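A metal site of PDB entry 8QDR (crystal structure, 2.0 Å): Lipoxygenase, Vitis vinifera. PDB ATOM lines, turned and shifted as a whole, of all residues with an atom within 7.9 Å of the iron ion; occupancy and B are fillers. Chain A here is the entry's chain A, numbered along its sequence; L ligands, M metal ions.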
ATOM      1  N   GLN A 517     -37.921  -8.078 -22.142  1.00  0.00           N
ATOM      2  CA  GLN A 517     -37.086  -9.050 -22.837  1.00  0.00           C
ATOM      3  C   GLN A 517     -36.481  -8.456 -24.121  1.00  0.00           C
ATOM      4  O   GLN A 517     -35.270  -8.542 -24.342  1.00  0.00           O
ATOM      5  CB  GLN A 517     -37.906 -10.311 -23.136  1.00  0.00           C
ATOM      6  CG  GLN A 517     -37.076 -11.536 -23.468  1.00  0.00           C
ATOM      7  CD  GLN A 517     -36.053 -11.878 -22.381  1.00  0.00           C
ATOM      8  OE1 GLN A 517     -36.252 -11.586 -21.195  1.00  0.00           O
ATOM      9  NE2 GLN A 517     -34.951 -12.501 -22.791  1.00  0.00           N
ATOM     10  N   HIS A 521     -33.669  -5.633 -22.146  1.00  0.00           N
ATOM     11  CA  HIS A 521     -32.651  -6.665 -22.058  1.00  0.00           C
ATOM     12  C   HIS A 521     -31.958  -6.852 -23.399  1.00  0.00           C
ATOM     13  O   HIS A 521     -30.824  -6.394 -23.556  1.00  0.00           O
ATOM     14  CB  HIS A 521     -33.280  -7.979 -21.582  1.00  0.00           C
ATOM     15  CG  HIS A 521     -32.292  -9.085 -21.419  1.00  0.00           C
ATOM     16  ND1 HIS A 521     -32.635 -10.416 -21.466  1.00  0.00           N
ATOM     17  CD2 HIS A 521     -30.951  -9.042 -21.218  1.00  0.00           C
ATOM     18  CE1 HIS A 521     -31.558 -11.148 -21.295  1.00  0.00           C
ATOM     19  NE2 HIS A 521     -30.518 -10.346 -21.143  1.00  0.00           N
ATOM     20  N   TRP A 522     -32.630  -7.467 -24.376  1.00  0.00           N
ATOM     21  CA  TRP A 522     -31.976  -7.781 -25.637  1.00  0.00           C
ATOM     22  C   TRP A 522     -31.398  -6.536 -26.309  1.00  0.00           C
ATOM     23  O   TRP A 522     -30.210  -6.481 -26.622  1.00  0.00           O
ATOM     24  CB  TRP A 522     -32.924  -8.500 -26.604  1.00  0.00           C
ATOM     25  CG  TRP A 522     -32.362  -8.505 -27.977  1.00  0.00           C
ATOM     26  CD1 TRP A 522     -32.802  -7.787 -29.049  1.00  0.00           C
ATOM     27  CD2 TRP A 522     -31.180  -9.196 -28.415  1.00  0.00           C
ATOM     28  NE1 TRP A 522     -32.000  -8.004 -30.137  1.00  0.00           N
ATOM     29  CE2 TRP A 522     -30.984  -8.863 -29.771  1.00  0.00           C
ATOM     30  CE3 TRP A 522     -30.275 -10.067 -27.788  1.00  0.00           C
ATOM     31  CZ2 TRP A 522     -29.918  -9.372 -30.527  1.00  0.00           C
ATOM     32  CZ3 TRP A 522     -29.210 -10.581 -28.536  1.00  0.00           C
ATOM     33  CH2 TRP A 522     -29.048 -10.228 -29.902  1.00  0.00           C
ATOM     34  N   THR A 525     -28.777  -4.019 -23.924  1.00  0.00           N
ATOM     35  CA  THR A 525     -27.503  -4.556 -23.458  1.00  0.00           C
ATOM     36  C   THR A 525     -26.845  -5.286 -24.629  1.00  0.00           C
ATOM     37  O   THR A 525     -25.992  -4.708 -25.303  1.00  0.00           O
ATOM     38  CB  THR A 525     -27.705  -5.451 -22.218  1.00  0.00           C
ATOM     39  OG1 THR A 525     -28.549  -6.561 -22.524  1.00  0.00           O
ATOM     40  CG2 THR A 525     -28.347  -4.644 -21.073  1.00  0.00           C
ATOM     41  N   HIS A 526     -27.292  -6.516 -24.926  1.00  0.00           N
ATOM     42  CA  HIS A 526     -26.703  -7.358 -25.973  1.00  0.00           C
ATOM     43  C   HIS A 526     -26.541  -6.652 -27.316  1.00  0.00           C
ATOM     44  O   HIS A 526     -25.447  -6.623 -27.902  1.00  0.00           O
ATOM     45  CB  HIS A 526     -27.571  -8.583 -26.170  1.00  0.00           C
ATOM     46  CG  HIS A 526     -27.573  -9.516 -25.017  1.00  0.00           C
ATOM     47  ND1 HIS A 526     -26.813 -10.656 -24.989  1.00  0.00           N
ATOM     48  CD2 HIS A 526     -28.222  -9.469 -23.823  1.00  0.00           C
ATOM     49  CE1 HIS A 526     -26.997 -11.281 -23.842  1.00  0.00           C
ATOM     50  NE2 HIS A 526     -27.837 -10.577 -23.112  1.00  0.00           N
ATOM     51  N   ILE A 560     -22.899 -15.216 -27.156  1.00  0.00           N
ATOM     52  CA  ILE A 560     -24.290 -15.285 -26.706  1.00  0.00           C
ATOM     53  C   ILE A 560     -25.215 -14.706 -27.768  1.00  0.00           C
ATOM     54  O   ILE A 560     -26.232 -15.303 -28.126  1.00  0.00           O
ATOM     55  CB  ILE A 560     -24.458 -14.560 -25.351  1.00  0.00           C
ATOM     56  CG1 ILE A 560     -23.709 -15.291 -24.252  1.00  0.00           C
ATOM     57  CG2 ILE A 560     -25.928 -14.484 -24.966  1.00  0.00           C
ATOM     58  CD1 ILE A 560     -24.328 -16.609 -23.869  1.00  0.00           C
ATOM     59  N   ASN A 561     -24.873 -13.521 -28.281  1.00  0.00           N
ATOM     60  CA  ASN A 561     -25.680 -12.915 -29.332  1.00  0.00           C
ATOM     61  C   ASN A 561     -25.799 -13.840 -30.536  1.00  0.00           C
ATOM     62  O   ASN A 561     -26.872 -13.963 -31.134  1.00  0.00           O
ATOM     63  CB  ASN A 561     -25.084 -11.574 -29.747  1.00  0.00           C
ATOM     64  CG  ASN A 561     -25.260 -10.518 -28.688  1.00  0.00           C
ATOM     65  OD1 ASN A 561     -25.754 -10.800 -27.590  1.00  0.00           O
ATOM     66  ND2 ASN A 561     -24.860  -9.300 -29.002  1.00  0.00           N
ATOM     67  N   HIS A 713     -27.076  -4.696 -17.299  1.00  0.00           N
ATOM     68  CA  HIS A 713     -27.402  -6.085 -17.631  1.00  0.00           C
ATOM     69  C   HIS A 713     -27.770  -6.890 -16.381  1.00  0.00           C
ATOM     70  O   HIS A 713     -28.736  -7.662 -16.404  1.00  0.00           O
ATOM     71  CB  HIS A 713     -26.248  -6.762 -18.381  1.00  0.00           C
ATOM     72  CG  HIS A 713     -26.606  -8.135 -18.862  1.00  0.00           C
ATOM     73  ND1 HIS A 713     -26.085  -9.285 -18.306  1.00  0.00           N
ATOM     74  CD2 HIS A 713     -27.470  -8.542 -19.820  1.00  0.00           C
ATOM     75  CE1 HIS A 713     -26.597 -10.340 -18.903  1.00  0.00           C
ATOM     76  NE2 HIS A 713     -27.436  -9.916 -19.836  1.00  0.00           N
ATOM     77  N   ALA A 714     -27.004  -6.735 -15.297  1.00  0.00           N
ATOM     78  CA  ALA A 714     -27.312  -7.439 -14.050  1.00  0.00           C
ATOM     79  C   ALA A 714     -28.730  -7.139 -13.556  1.00  0.00           C
ATOM     80  O   ALA A 714     -29.442  -8.036 -13.086  1.00  0.00           O
ATOM     81  CB  ALA A 714     -26.281  -7.090 -12.972  1.00  0.00           C
ATOM     82  N   VAL A 716     -31.483  -6.317 -15.167  1.00  0.00           N
ATOM     83  CA  VAL A 716     -32.617  -6.824 -15.952  1.00  0.00           C
ATOM     84  C   VAL A 716     -32.554  -8.319 -16.220  1.00  0.00           C
ATOM     85  O   VAL A 716     -33.513  -8.873 -16.774  1.00  0.00           O
ATOM     86  CB  VAL A 716     -32.759  -6.086 -17.310  1.00  0.00           C
ATOM     87  CG1 VAL A 716     -32.953  -4.587 -17.092  1.00  0.00           C
ATOM     88  CG2 VAL A 716     -31.568  -6.409 -18.232  1.00  0.00           C
ATOM     89  N   ASN A 717     -31.466  -8.992 -15.856  1.00  0.00           N
ATOM     90  CA  ASN A 717     -31.293 -10.385 -16.232  1.00  0.00           C
ATOM     91  C   ASN A 717     -31.363 -11.313 -15.016  1.00  0.00           C
ATOM     92  O   ASN A 717     -32.321 -12.084 -14.890  1.00  0.00           O
ATOM     93  CB  ASN A 717     -29.981 -10.575 -16.993  1.00  0.00           C
ATOM     94  CG  ASN A 717     -29.905 -11.914 -17.701  1.00  0.00           C
ATOM     95  OD1 ASN A 717     -28.937 -12.662 -17.534  1.00  0.00           O
ATOM     96  ND2 ASN A 717     -30.930 -12.221 -18.494  1.00  0.00           N
ATOM     97  N   PHE A 718     -30.384 -11.254 -14.118  1.00  0.00           N
ATOM     98  CA  PHE A 718     -30.297 -12.197 -13.008  1.00  0.00           C
ATOM     99  C   PHE A 718     -31.439 -12.031 -12.015  1.00  0.00           C
ATOM    100  O   PHE A 718     -32.418 -12.777 -12.069  1.00  0.00           O
ATOM    101  CB  PHE A 718     -28.956 -12.035 -12.284  1.00  0.00           C
ATOM    102  CG  PHE A 718     -27.767 -12.216 -13.185  1.00  0.00           C
ATOM    103  CD1 PHE A 718     -27.198 -11.126 -13.816  1.00  0.00           C
ATOM    104  CD2 PHE A 718     -27.246 -13.480 -13.411  1.00  0.00           C
ATOM    105  CE1 PHE A 718     -26.119 -11.298 -14.661  1.00  0.00           C
ATOM    106  CE2 PHE A 718     -26.167 -13.651 -14.256  1.00  0.00           C
ATOM    107  CZ  PHE A 718     -25.609 -12.560 -14.875  1.00  0.00           C
ATOM    108  N   VAL A 778     -30.759 -20.422 -18.285  1.00  0.00           N
ATOM    109  CA  VAL A 778     -29.380 -20.111 -18.625  1.00  0.00           C
ATOM    110  C   VAL A 778     -29.173 -18.603 -18.771  1.00  0.00           C
ATOM    111  O   VAL A 778     -30.115 -17.846 -19.025  1.00  0.00           O
ATOM    112  CB  VAL A 778     -28.938 -20.849 -19.906  1.00  0.00           C
ATOM    113  CG1 VAL A 778     -29.662 -22.191 -20.036  1.00  0.00           C
ATOM    114  CG2 VAL A 778     -29.164 -19.971 -21.138  1.00  0.00           C
ATOM    115  N   SER A 860     -19.357  -8.333 -17.571  1.00  0.00           N
ATOM    116  CA  SER A 860     -19.771  -8.331 -18.972  1.00  0.00           C
ATOM    117  C   SER A 860     -21.160  -8.951 -19.135  1.00  0.00           C
ATOM    118  O   SER A 860     -21.680  -9.631 -18.244  1.00  0.00           O
ATOM    119  CB  SER A 860     -18.796  -9.122 -19.858  1.00  0.00           C
ATOM    120  OG  SER A 860     -19.026 -10.515 -19.738  1.00  0.00           O
ATOM    121  N   ILE A 861     -21.753  -8.705 -20.302  1.00  0.00           N
ATOM    122  CA  ILE A 861     -22.987  -9.373 -20.703  1.00  0.00           C
ATOM    123  C   ILE A 861     -22.631 -10.817 -21.046  1.00  0.00           C
ATOM    124  O   ILE A 861     -22.199 -11.118 -22.166  1.00  0.00           O
ATOM    125  CB  ILE A 861     -23.641  -8.626 -21.888  1.00  0.00           C
ATOM    126  CG1 ILE A 861     -23.851  -7.154 -21.525  1.00  0.00           C
ATOM    127  CG2 ILE A 861     -24.977  -9.258 -22.277  1.00  0.00           C
ATOM    128  CD1 ILE A 861     -24.228  -6.312 -22.702  1.00  0.00           C
ATOM    129  N   SER A 862     -22.780 -11.713 -20.071  1.00  0.00           N
ATOM    130  CA  SER A 862     -22.222 -13.055 -20.160  1.00  0.00           C
ATOM    131  C   SER A 862     -23.280 -14.132 -20.336  1.00  0.00           C
ATOM    132  O   SER A 862     -22.947 -15.317 -20.375  1.00  0.00           O
ATOM    133  CB  SER A 862     -21.378 -13.348 -18.914  1.00  0.00           C
ATOM    134  OG  SER A 862     -22.177 -13.399 -17.745  1.00  0.00           O
ATOM    135  N   ILE A 863     -24.548 -13.758 -20.447  1.00  0.00           N
ATOM    136  CA  ILE A 863     -25.616 -14.744 -20.515  1.00  0.00           C
ATOM    137  C   ILE A 863     -26.903 -14.068 -20.961  1.00  0.00           C
ATOM    138  O   ILE A 863     -27.899 -14.705 -21.343  1.00  0.00           O
ATOM    139  CB  ILE A 863     -25.774 -15.473 -19.151  1.00  0.00           C
ATOM    140  CG1 ILE A 863     -26.425 -16.846 -19.336  1.00  0.00           C
ATOM    141  CG2 ILE A 863     -26.531 -14.599 -18.160  1.00  0.00           C
ATOM    142  CD1 ILE A 863     -25.561 -17.822 -20.114  1.00  0.00           C
ATOM    143  OXT ILE A 863     -26.978 -12.832 -20.950  1.00  0.00           O
HETATM  144  C1  LIG L   1     -29.497 -13.359 -23.761  1.00  0.00           C
HETATM  145  O1  LIG L   1     -29.739 -13.552 -22.361  1.00  0.00           O
HETATM  146  C2  LIG L   1     -30.743 -13.684 -24.567  1.00  0.00           C
HETATM  147  O2  LIG L   1     -31.852 -12.918 -24.101  1.00  0.00           O
HETATM  148 FE    FE M   1     -28.661 -11.350 -21.198  1.00  0.00          FE
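Merely in contact with the iron ion: Asn 717 (3.6 Å).
Within 4 Å of the iron ion: His 521, His 526, His 713, Asn 717 and Ile 863.
The nearest printed residue that does not touch the iron ion is Ile 861 (4.4 Å).
The iron ion is bound by NE2 of His 521 (2.1 Å), NE2 of His 526 (2.2 Å), OXT of Ile 863 (2.3 Å) and NE2 of His 713 (2.3 Å).
The iron ion has four donor atoms within binding distance.
Slightly farther from the iron ion lies an oxygen (O1) of the ligand (2.7 Å).
A ring nitrogen (NE2) of His 521 lies close to the side-chain amide nitrogen (ND2) of Asn 717.
A ring nitrogen (ND1) of His 521 lies within hydrogen-bond range of the side-chain amide nitrogen (NE2) of Gln 517, at 3.4 Å.
A ring nitrogen (ND1) of His 526 lies within hydrogen-bond range of the side-chain amide oxygen (OD1) of Asn 561 (2.8 Å).
The backbone carbonyl oxygen (O) of His 521 lies within hydrogen-bond range of the side-chain hydroxyl (OG1) of Thr 525 (2.5 Å).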
